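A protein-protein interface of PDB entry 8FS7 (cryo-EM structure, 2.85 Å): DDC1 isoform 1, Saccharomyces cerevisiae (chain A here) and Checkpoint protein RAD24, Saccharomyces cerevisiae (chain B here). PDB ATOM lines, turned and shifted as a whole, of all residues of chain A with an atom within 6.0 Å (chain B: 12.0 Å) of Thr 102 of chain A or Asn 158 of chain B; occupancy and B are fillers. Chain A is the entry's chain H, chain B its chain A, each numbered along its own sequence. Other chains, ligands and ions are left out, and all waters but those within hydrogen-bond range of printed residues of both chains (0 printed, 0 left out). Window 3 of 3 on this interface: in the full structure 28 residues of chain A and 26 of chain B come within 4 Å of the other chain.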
ATOM      1  N   PHE A  17      -0.833  10.063  13.402  1.00  0.00           N
ATOM      2  CA  PHE A  17      -0.939  11.253  14.240  1.00  0.00           C
ATOM      3  C   PHE A  17      -1.593  10.934  15.577  1.00  0.00           C
ATOM      4  O   PHE A  17      -1.157  11.432  16.621  1.00  0.00           O
ATOM      5  CB  PHE A  17      -1.722  12.344  13.511  1.00  0.00           C
ATOM      6  CG  PHE A  17      -2.255  13.415  14.420  1.00  0.00           C
ATOM      7  CD1 PHE A  17      -1.395  14.311  15.034  1.00  0.00           C
ATOM      8  CD2 PHE A  17      -3.614  13.524  14.662  1.00  0.00           C
ATOM      9  CE1 PHE A  17      -1.883  15.297  15.872  1.00  0.00           C
ATOM     10  CE2 PHE A  17      -4.107  14.507  15.500  1.00  0.00           C
ATOM     11  CZ  PHE A  17      -3.239  15.394  16.105  1.00  0.00           C
ATOM     12  N   ILE A  20       0.917   9.071  17.756  1.00  0.00           N
ATOM     13  CA  ILE A  20       1.935   9.987  18.267  1.00  0.00           C
ATOM     14  C   ILE A  20       1.363  10.853  19.384  1.00  0.00           C
ATOM     15  O   ILE A  20       2.010  11.068  20.418  1.00  0.00           O
ATOM     16  CB  ILE A  20       2.511  10.839  17.121  1.00  0.00           C
ATOM     17  CG1 ILE A  20       3.346   9.967  16.180  1.00  0.00           C
ATOM     18  CG2 ILE A  20       3.353  11.981  17.665  1.00  0.00           C
ATOM     19  CD1 ILE A  20       4.458   9.210  16.874  1.00  0.00           C
ATOM     20  N   TYR A  21       0.137  11.351  19.202  1.00  0.00           N
ATOM     21  CA  TYR A  21      -0.497  12.170  20.231  1.00  0.00           C
ATOM     22  C   TYR A  21      -0.702  11.382  21.520  1.00  0.00           C
ATOM     23  O   TYR A  21      -0.464  11.900  22.617  1.00  0.00           O
ATOM     24  CB  TYR A  21      -1.828  12.717  19.716  1.00  0.00           C
ATOM     25  CG  TYR A  21      -2.617  13.500  20.742  1.00  0.00           C
ATOM     26  CD1 TYR A  21      -2.333  14.836  20.993  1.00  0.00           C
ATOM     27  CD2 TYR A  21      -3.655  12.908  21.452  1.00  0.00           C
ATOM     28  CE1 TYR A  21      -3.053  15.557  21.927  1.00  0.00           C
ATOM     29  CE2 TYR A  21      -4.380  13.619  22.387  1.00  0.00           C
ATOM     30  CZ  TYR A  21      -4.075  14.943  22.621  1.00  0.00           C
ATOM     31  OH  TYR A  21      -4.795  15.657  23.551  1.00  0.00           O
ATOM     32  N   VAL A  22      -1.138  10.128  21.409  1.00  0.00           N
ATOM     33  CA  VAL A  22      -1.360   9.317  22.602  1.00  0.00           C
ATOM     34  C   VAL A  22      -0.041   9.011  23.305  1.00  0.00           C
ATOM     35  O   VAL A  22       0.054   9.090  24.539  1.00  0.00           O
ATOM     36  CB  VAL A  22      -2.132   8.039  22.235  1.00  0.00           C
ATOM     37  CG1 VAL A  22      -2.000   6.994  23.330  1.00  0.00           C
ATOM     38  CG2 VAL A  22      -3.592   8.386  21.996  1.00  0.00           C
ATOM     39  N   SER A  24       2.508  10.870  23.280  1.00  0.00           N
ATOM     40  CA  SER A  24       2.843  12.112  23.969  1.00  0.00           C
ATOM     41  C   SER A  24       2.043  12.271  25.257  1.00  0.00           C
ATOM     42  O   SER A  24       2.579  12.750  26.262  1.00  0.00           O
ATOM     43  CB  SER A  24       2.606  13.307  23.046  1.00  0.00           C
ATOM     44  OG  SER A  24       1.223  13.504  22.809  1.00  0.00           O
ATOM     45  N   THR A  25       0.764  11.883  25.245  1.00  0.00           N
ATOM     46  CA  THR A  25      -0.048  11.956  26.458  1.00  0.00           C
ATOM     47  C   THR A  25       0.355  10.913  27.491  1.00  0.00           C
ATOM     48  O   THR A  25      -0.112  10.978  28.632  1.00  0.00           O
ATOM     49  CB  THR A  25      -1.536  11.786  26.137  1.00  0.00           C
ATOM     50  OG1 THR A  25      -1.760  10.499  25.550  1.00  0.00           O
ATOM     51  CG2 THR A  25      -2.016  12.871  25.188  1.00  0.00           C
ATOM     52  N   ASP A  28       6.224  12.703  28.191  1.00  0.00           N
ATOM     53  CA  ASP A  28       6.609  13.906  27.461  1.00  0.00           C
ATOM     54  C   ASP A  28       7.581  13.626  26.320  1.00  0.00           C
ATOM     55  O   ASP A  28       7.696  14.453  25.410  1.00  0.00           O
ATOM     56  CB  ASP A  28       7.224  14.925  28.422  1.00  0.00           C
ATOM     57  CG  ASP A  28       8.568  14.479  28.962  1.00  0.00           C
ATOM     58  OD1 ASP A  28       8.688  13.301  29.362  1.00  0.00           O
ATOM     59  OD2 ASP A  28       9.504  15.305  28.989  1.00  0.00           O
ATOM     60  N   ILE A  30       8.802  10.740  23.351  1.00  0.00           N
ATOM     61  CA  ILE A  30       8.428   9.535  22.620  1.00  0.00           C
ATOM     62  C   ILE A  30       9.690   8.816  22.167  1.00  0.00           C
ATOM     63  O   ILE A  30      10.611   9.430  21.616  1.00  0.00           O
ATOM     64  CB  ILE A  30       7.522   9.879  21.423  1.00  0.00           C
ATOM     65  CG1 ILE A  30       6.199  10.472  21.905  1.00  0.00           C
ATOM     66  CG2 ILE A  30       7.267   8.647  20.565  1.00  0.00           C
ATOM     67  CD1 ILE A  30       5.244  10.809  20.784  1.00  0.00           C
ATOM     68  N   ASN A  97      10.803  14.529  21.364  1.00  0.00           N
ATOM     69  CA  ASN A  97       9.784  15.177  22.177  1.00  0.00           C
ATOM     70  C   ASN A  97       8.394  14.834  21.653  1.00  0.00           C
ATOM     71  O   ASN A  97       8.131  14.926  20.450  1.00  0.00           O
ATOM     72  CB  ASN A  97       9.994  16.691  22.179  1.00  0.00           C
ATOM     73  CG  ASN A  97       9.212  17.393  23.276  1.00  0.00           C
ATOM     74  OD1 ASN A  97       8.349  16.799  23.921  1.00  0.00           O
ATOM     75  ND2 ASN A  97       9.513  18.666  23.492  1.00  0.00           N
ATOM     76  N   GLY A  98       7.504  14.434  22.563  1.00  0.00           N
ATOM     77  CA  GLY A  98       6.152  14.082  22.160  1.00  0.00           C
ATOM     78  C   GLY A  98       5.352  15.266  21.654  1.00  0.00           C
ATOM     79  O   GLY A  98       4.663  15.170  20.634  1.00  0.00           O
ATOM     80  N   ARG A  99       5.425  16.398  22.359  1.00  0.00           N
ATOM     81  CA  ARG A  99       4.669  17.577  21.948  1.00  0.00           C
ATOM     82  C   ARG A  99       5.190  18.139  20.632  1.00  0.00           C
ATOM     83  O   ARG A  99       4.406  18.603  19.796  1.00  0.00           O
ATOM     84  CB  ARG A  99       4.717  18.640  23.046  1.00  0.00           C
ATOM     85  CG  ARG A  99       3.997  18.241  24.323  1.00  0.00           C
ATOM     86  CD  ARG A  99       3.874  19.411  25.287  1.00  0.00           C
ATOM     87  NE  ARG A  99       5.140  19.721  25.939  1.00  0.00           N
ATOM     88  CZ  ARG A  99       5.938  20.722  25.592  1.00  0.00           C
ATOM     89  NH1 ARG A  99       5.629  21.539  24.598  1.00  0.00           N
ATOM     90  NH2 ARG A  99       7.074  20.909  26.259  1.00  0.00           N
ATOM     91  N   HIS A 100       6.510  18.118  20.436  1.00  0.00           N
ATOM     92  CA  HIS A 100       7.077  18.590  19.178  1.00  0.00           C
ATOM     93  C   HIS A 100       6.690  17.682  18.017  1.00  0.00           C
ATOM     94  O   HIS A 100       6.444  18.159  16.903  1.00  0.00           O
ATOM     95  CB  HIS A 100       8.597  18.698  19.294  1.00  0.00           C
ATOM     96  CG  HIS A 100       9.057  19.798  20.198  1.00  0.00           C
ATOM     97  ND1 HIS A 100      10.323  19.837  20.740  1.00  0.00           N
ATOM     98  CD2 HIS A 100       8.418  20.901  20.655  1.00  0.00           C
ATOM     99  CE1 HIS A 100      10.446  20.917  21.491  1.00  0.00           C
ATOM    100  NE2 HIS A 100       9.303  21.579  21.457  1.00  0.00           N
ATOM    101  N   LEU A 101       6.640  16.369  18.252  1.00  0.00           N
ATOM    102  CA  LEU A 101       6.294  15.446  17.176  1.00  0.00           C
ATOM    103  C   LEU A 101       4.805  15.478  16.855  1.00  0.00           C
ATOM    104  O   LEU A 101       4.424  15.325  15.689  1.00  0.00           O
ATOM    105  CB  LEU A 101       6.729  14.026  17.539  1.00  0.00           C
ATOM    106  CG  LEU A 101       6.745  13.021  16.385  1.00  0.00           C
ATOM    107  CD1 LEU A 101       7.584  13.543  15.229  1.00  0.00           C
ATOM    108  CD2 LEU A 101       7.255  11.669  16.853  1.00  0.00           C
ATOM    109  N   THR A 102       3.951  15.671  17.862  1.00  0.00           N
ATOM    110  CA  THR A 102       2.511  15.652  17.630  1.00  0.00           C
ATOM    111  C   THR A 102       1.998  16.933  16.982  1.00  0.00           C
ATOM    112  O   THR A 102       0.889  16.930  16.437  1.00  0.00           O
ATOM    113  CB  THR A 102       1.762  15.402  18.942  1.00  0.00           C
ATOM    114  OG1 THR A 102       0.415  15.008  18.656  1.00  0.00           O
ATOM    115  CG2 THR A 102       1.743  16.656  19.799  1.00  0.00           C
ATOM    116  N   THR A 103       2.767  18.019  17.027  1.00  0.00           N
ATOM    117  CA  THR A 103       2.400  19.253  16.344  1.00  0.00           C
ATOM    118  C   THR A 103       2.911  19.293  14.911  1.00  0.00           C
ATOM    119  O   THR A 103       2.626  20.255  14.190  1.00  0.00           O
ATOM    120  CB  THR A 103       2.920  20.469  17.121  1.00  0.00           C
ATOM    121  OG1 THR A 103       2.203  21.641  16.716  1.00  0.00           O
ATOM    122  CG2 THR A 103       4.406  20.677  16.868  1.00  0.00           C
ATOM    123  N   ILE A 104       3.653  18.275  14.489  1.00  0.00           N
ATOM    124  CA  ILE A 104       4.138  18.172  13.118  1.00  0.00           C
ATOM    125  C   ILE A 104       3.221  17.301  12.272  1.00  0.00           C
ATOM    126  O   ILE A 104       2.878  17.652  11.139  1.00  0.00           O
ATOM    127  CB  ILE A 104       5.584  17.630  13.123  1.00  0.00           C
ATOM    128  CG1 ILE A 104       6.550  18.679  13.676  1.00  0.00           C
ATOM    129  CG2 ILE A 104       5.997  17.172  11.737  1.00  0.00           C
ATOM    130  CD1 ILE A 104       7.982  18.204  13.737  1.00  0.00           C
ATOM    131  N   SER A 105       2.797  16.163  12.818  1.00  0.00           N
ATOM    132  CA  SER A 105       1.999  15.188  12.087  1.00  0.00           C
ATOM    133  C   SER A 105       0.513  15.519  12.071  1.00  0.00           C
ATOM    134  O   SER A 105      -0.267  14.747  11.504  1.00  0.00           O
ATOM    135  CB  SER A 105       2.207  13.794  12.683  1.00  0.00           C
ATOM    136  OG  SER A 105       1.945  13.792  14.076  1.00  0.00           O
ATOM    137  N   ARG A 106       0.103  16.628  12.680  1.00  0.00           N
ATOM    138  CA  ARG A 106      -1.298  17.016  12.675  1.00  0.00           C
ATOM    139  C   ARG A 106      -1.756  17.365  11.262  1.00  0.00           C
ATOM    140  O   ARG A 106      -0.982  17.834  10.422  1.00  0.00           O
ATOM    141  CB  ARG A 106      -1.529  18.208  13.603  1.00  0.00           C
ATOM    142  CG  ARG A 106      -0.401  19.222  13.584  1.00  0.00           C
ATOM    143  CD  ARG A 106      -0.903  20.621  13.885  1.00  0.00           C
ATOM    144  NE  ARG A 106      -1.489  21.246  12.705  1.00  0.00           N
ATOM    145  CZ  ARG A 106      -0.800  21.917  11.793  1.00  0.00           C
ATOM    146  NH1 ARG A 106       0.511  22.073  11.894  1.00  0.00           N
ATOM    147  NH2 ARG A 106      -1.440  22.445  10.754  1.00  0.00           N
ATOM    148  N   ARG B 152       9.145  13.560  39.026  1.00  0.00           N
ATOM    149  CA  ARG B 152       9.851  14.481  38.141  1.00  0.00           C
ATOM    150  C   ARG B 152       8.862  15.549  37.699  1.00  0.00           C
ATOM    151  O   ARG B 152       7.910  15.257  36.970  1.00  0.00           O
ATOM    152  CB  ARG B 152      10.456  13.737  36.948  1.00  0.00           C
ATOM    153  CG  ARG B 152      11.581  14.481  36.254  1.00  0.00           C
ATOM    154  CD  ARG B 152      11.928  13.856  34.910  1.00  0.00           C
ATOM    155  NE  ARG B 152      11.527  14.689  33.782  1.00  0.00           N
ATOM    156  CZ  ARG B 152      10.821  14.255  32.747  1.00  0.00           C
ATOM    157  NH1 ARG B 152      10.419  12.997  32.662  1.00  0.00           N
ATOM    158  NH2 ARG B 152      10.516  15.103  31.768  1.00  0.00           N
ATOM    159  N   GLY B 153       9.086  16.787  38.147  1.00  0.00           N
ATOM    160  CA  GLY B 153       8.081  17.822  37.969  1.00  0.00           C
ATOM    161  C   GLY B 153       8.119  18.480  36.603  1.00  0.00           C
ATOM    162  O   GLY B 153       7.121  19.048  36.152  1.00  0.00           O
ATOM    163  N   ASP B 154       9.267  18.419  35.924  1.00  0.00           N
ATOM    164  CA  ASP B 154       9.395  19.127  34.654  1.00  0.00           C
ATOM    165  C   ASP B 154       8.743  18.375  33.501  1.00  0.00           C
ATOM    166  O   ASP B 154       8.676  18.910  32.389  1.00  0.00           O
ATOM    167  CB  ASP B 154      10.871  19.405  34.346  1.00  0.00           C
ATOM    168  CG  ASP B 154      11.744  18.175  34.483  1.00  0.00           C
ATOM    169  OD1 ASP B 154      11.200  17.056  34.536  1.00  0.00           O
ATOM    170  OD2 ASP B 154      12.982  18.330  34.542  1.00  0.00           O
ATOM    171  N   CYS B 155       8.269  17.154  33.734  1.00  0.00           N
ATOM    172  CA  CYS B 155       7.573  16.401  32.699  1.00  0.00           C
ATOM    173  C   CYS B 155       6.254  17.071  32.344  1.00  0.00           C
ATOM    174  O   CYS B 155       5.372  17.220  33.195  1.00  0.00           O
ATOM    175  CB  CYS B 155       7.331  14.966  33.173  1.00  0.00           C
ATOM    176  SG  CYS B 155       6.462  13.918  31.981  1.00  0.00           S
ATOM    177  N   ILE B 156       6.122  17.477  31.085  1.00  0.00           N
ATOM    178  CA  ILE B 156       4.926  18.149  30.590  1.00  0.00           C
ATOM    179  C   ILE B 156       4.228  17.180  29.645  1.00  0.00           C
ATOM    180  O   ILE B 156       4.639  17.013  28.490  1.00  0.00           O
ATOM    181  CB  ILE B 156       5.249  19.476  29.893  1.00  0.00           C
ATOM    182  CG1 ILE B 156       5.920  20.438  30.874  1.00  0.00           C
ATOM    183  CG2 ILE B 156       3.982  20.101  29.325  1.00  0.00           C
ATOM    184  CD1 ILE B 156       6.250  21.787  30.276  1.00  0.00           C
ATOM    185  N   VAL B 157       3.174  16.534  30.136  1.00  0.00           N
ATOM    186  CA  VAL B 157       2.396  15.618  29.315  1.00  0.00           C
ATOM    187  C   VAL B 157       1.297  16.390  28.589  1.00  0.00           C
ATOM    188  O   VAL B 157       0.727  17.350  29.115  1.00  0.00           O
ATOM    189  CB  VAL B 157       1.828  14.475  30.182  1.00  0.00           C
ATOM    190  CG1 VAL B 157       0.539  13.908  29.608  1.00  0.00           C
ATOM    191  CG2 VAL B 157       2.867  13.376  30.354  1.00  0.00           C
ATOM    192  N   ASN B 158       1.030  15.979  27.342  1.00  0.00           N
ATOM    193  CA  ASN B 158       0.070  16.683  26.491  1.00  0.00           C
ATOM    194  C   ASN B 158      -1.292  16.822  27.164  1.00  0.00           C
ATOM    195  O   ASN B 158      -1.793  17.937  27.348  1.00  0.00           O
ATOM    196  CB  ASN B 158      -0.068  15.950  25.157  1.00  0.00           C
ATOM    197  CG  ASN B 158       0.269  16.826  23.972  1.00  0.00           C
ATOM    198  OD1 ASN B 158       0.201  18.052  24.048  1.00  0.00           O
ATOM    199  ND2 ASN B 158       0.635  16.198  22.862  1.00  0.00           N
ATOM    200  N   ASP B 159      -1.909  15.701  27.537  1.00  0.00           N
ATOM    201  CA  ASP B 159      -3.228  15.719  28.169  1.00  0.00           C
ATOM    202  C   ASP B 159      -3.027  15.631  29.680  1.00  0.00           C
ATOM    203  O   ASP B 159      -3.414  14.666  30.339  1.00  0.00           O
ATOM    204  CB  ASP B 159      -4.101  14.586  27.632  1.00  0.00           C
ATOM    205  CG  ASP B 159      -5.508  14.601  28.205  1.00  0.00           C
ATOM    206  OD1 ASP B 159      -5.910  15.631  28.786  1.00  0.00           O
ATOM    207  OD2 ASP B 159      -6.212  13.578  28.075  1.00  0.00           O
ATOM    208  N   LEU B 160      -2.394  16.664  30.228  1.00  0.00           N
ATOM    209  CA  LEU B 160      -2.176  16.758  31.666  1.00  0.00           C
ATOM    210  C   LEU B 160      -2.055  18.211  32.103  1.00  0.00           C
ATOM    211  O   LEU B 160      -1.031  18.854  31.842  1.00  0.00           O
ATOM    212  CB  LEU B 160      -0.929  15.983  32.087  1.00  0.00           C
ATOM    213  CG  LEU B 160      -0.996  15.313  33.460  1.00  0.00           C
ATOM    214  CD1 LEU B 160      -2.071  14.246  33.481  1.00  0.00           C
ATOM    215  CD2 LEU B 160       0.354  14.721  33.825  1.00  0.00           C
ATOM    216  N   PRO B 161      -3.078  18.763  32.752  1.00  0.00           N
ATOM    217  CA  PRO B 161      -2.921  20.072  33.391  1.00  0.00           C
ATOM    218  C   PRO B 161      -1.836  20.013  34.457  1.00  0.00           C
ATOM    219  O   PRO B 161      -1.587  18.966  35.059  1.00  0.00           O
ATOM    220  CB  PRO B 161      -4.304  20.337  33.998  1.00  0.00           C
ATOM    221  CG  PRO B 161      -5.238  19.497  33.189  1.00  0.00           C
ATOM    222  CD  PRO B 161      -4.461  18.264  32.839  1.00  0.00           C
ATOM    223  N   GLN B 162      -1.176  21.154  34.672  1.00  0.00           N
ATOM    224  CA  GLN B 162       0.009  21.183  35.526  1.00  0.00           C
ATOM    225  C   GLN B 162      -0.317  20.790  36.962  1.00  0.00           C
ATOM    226  O   GLN B 162       0.468  20.089  37.613  1.00  0.00           O
ATOM    227  CB  GLN B 162       0.651  22.569  35.481  1.00  0.00           C
ATOM    228  CG  GLN B 162       1.922  22.638  34.648  1.00  0.00           C
ATOM    229  CD  GLN B 162       2.860  21.478  34.920  1.00  0.00           C
ATOM    230  OE1 GLN B 162       3.015  20.583  34.090  1.00  0.00           O
ATOM    231  NE2 GLN B 162       3.491  21.489  36.088  1.00  0.00           N
ATOM    232  N   MET B 163      -1.468  21.229  37.477  1.00  0.00           N
ATOM    233  CA  MET B 163      -1.853  20.863  38.836  1.00  0.00           C
ATOM    234  C   MET B 163      -2.224  19.391  38.959  1.00  0.00           C
ATOM    235  O   MET B 163      -2.187  18.847  40.067  1.00  0.00           O
ATOM    236  CB  MET B 163      -3.021  21.732  39.306  1.00  0.00           C
ATOM    237  CG  MET B 163      -2.656  23.187  39.544  1.00  0.00           C
ATOM    238  SD  MET B 163      -4.010  24.185  40.200  1.00  0.00           S
ATOM    239  CE  MET B 163      -5.304  22.963  40.407  1.00  0.00           C
ATOM    240  N   GLU B 164      -2.576  18.738  37.853  1.00  0.00           N
ATOM    241  CA  GLU B 164      -2.946  17.330  37.870  1.00  0.00           C
ATOM    242  C   GLU B 164      -1.755  16.396  37.700  1.00  0.00           C
ATOM    243  O   GLU B 164      -1.929  15.176  37.793  1.00  0.00           O
ATOM    244  CB  GLU B 164      -3.974  17.042  36.769  1.00  0.00           C
ATOM    245  CG  GLU B 164      -5.341  17.659  37.015  1.00  0.00           C
ATOM    246  CD  GLU B 164      -5.849  17.412  38.421  1.00  0.00           C
ATOM    247  OE1 GLU B 164      -5.991  16.232  38.805  1.00  0.00           O
ATOM    248  OE2 GLU B 164      -6.105  18.399  39.143  1.00  0.00           O
ATOM    249  N   SER B 165      -0.558  16.937  37.454  1.00  0.00           N
ATOM    250  CA  SER B 165       0.613  16.092  37.242  1.00  0.00           C
ATOM    251  C   SER B 165       0.961  15.304  38.498  1.00  0.00           C
ATOM    252  O   SER B 165       1.228  14.098  38.434  1.00  0.00           O
ATOM    253  CB  SER B 165       1.799  16.947  36.794  1.00  0.00           C
ATOM    254  OG  SER B 165       2.340  17.676  37.880  1.00  0.00           O
ATOM    255  N   GLU B 168      -1.688  12.579  39.086  1.00  0.00           N
ATOM    256  CA  GLU B 168      -1.460  11.432  38.213  1.00  0.00           C
ATOM    257  C   GLU B 168      -0.255  10.622  38.674  1.00  0.00           C
ATOM    258  O   GLU B 168      -0.279   9.386  38.635  1.00  0.00           O
ATOM    259  CB  GLU B 168      -1.274  11.900  36.769  1.00  0.00           C
ATOM    260  CG  GLU B 168      -1.545  10.823  35.730  1.00  0.00           C
ATOM    261  CD  GLU B 168      -2.998  10.393  35.697  1.00  0.00           C
ATOM    262  OE1 GLU B 168      -3.878  11.236  35.972  1.00  0.00           O
ATOM    263  OE2 GLU B 168      -3.262   9.210  35.395  1.00  0.00           O
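Tyr 21 of chain A touches Asn 158 of chain B. Val 157 of chain B touches Thr 25 of chain A (CG1 to O, 3.2 Å). Thr 25 of chain A touches Asn 158 of chain B (CG2 to CB, 3.6 Å). Asp 159 of chain B touches Thr 25 of chain A (CB to CG2, 3.6 Å). Ile 156 of chain B touches Asp 28 of chain A (O to CB, 3.3 Å). Arg 99 of chain A touches Ile 156 of chain B (NE to CG2, 3.6 Å). Asn 158 of chain B touches Arg 99 of chain A (OD1 to CG, 3.8 Å). Asn 158 of chain B touches Thr 102 of chain A (ND2 to CG2, 3.3 Å).
Of the printed residues of chain A, Asn 158 of chain B touches Tyr 21 (3.8 Å), Ser 24 (2.8 Å), Thr 25 (3.6 Å), Arg 99 (3.8 Å) and Thr 102 (3.3 Å). Phe 17 of chain A touches none of the printed residues of chain B. No residue of chain B comes within 4 Å of Ile 20 of chain A. Tyr 21 of chain A touches just one residue of chain B: Asn 158 (3.8 Å). Of chain B, only Asn 158 (2.8 Å) comes within 4 Å of Ser 24 of chain A. Ser 105 of chain A touches none of the printed residues of chain B. Printed residues of chain B within 4 Å of Asp 28 of chain A: Arg 152 (3.0 Å), Cys 155 (3.5 Å) and Ile 156 (3.3 Å). Printed residues of chain A within 4 Å of Val 157 of chain B: Thr 25 (3.2 Å). Printed residues of chain A within 4 Å of Asp 159 of chain B: Thr 25. The nearest residue of chain B that does not touch Thr 102 of chain A is Asp 159 of chain B (8.6 Å). The nearest residue of chain A that does not touch Asn 158 of chain B is Gly 98 of chain A (4.7 Å).
NH2 of Arg 152 of chain B is in salt-bridge range of OD2 of Asp 28 of chain A. The side-chain hydroxyl (OG) of Ser 24 of chain A is in hydrogen-bond range of the side-chain amide nitrogen (ND2) of Asn 158 of chain B. The side-chain carboxylate (OD1) of Asp 28 of chain A sits at hydrogen-bond distance from the side-chain sulfur (SG) of Cys 155 of chain B (3.5 Å).
Of the 15 printed residues of chain B, 6 touch a printed residue of chain A. Hydrophobic or aromatic side chains of chain B that line the printed part of chain A: Ile 156 and Val 157. Among the printed residues, 11 pairs touch across the chains.
O of Tyr 21 of chain A lies close to OG1 of Thr 25 of chain A, at 3.5 Å. N of Arg 99 of chain A sits at hydrogen-bond distance from OD1 of Asn 97 of chain A, 3.3 Å away. The guanidinium group (NE) of Arg 152 of chain B is in salt-bridge range of the side-chain carboxylate (OD1) of Asp 154 of chain B (2.5 Å). The backbone carbonyl oxygen of Asp 28 of chain A lies close to the side-chain amide oxygen of Asn 97 of chain A (2.9 Å). The side-chain hydroxyl (OG1) of Thr 25 of chain A is in hydrogen-bond range of the backbone carbonyl oxygen (O) of Val 22 of chain A. The backbone carbonyl oxygen of Asp 28 of chain A sits at hydrogen-bond distance from the backbone NH of Gly 98 of chain A, 2.9 Å away.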
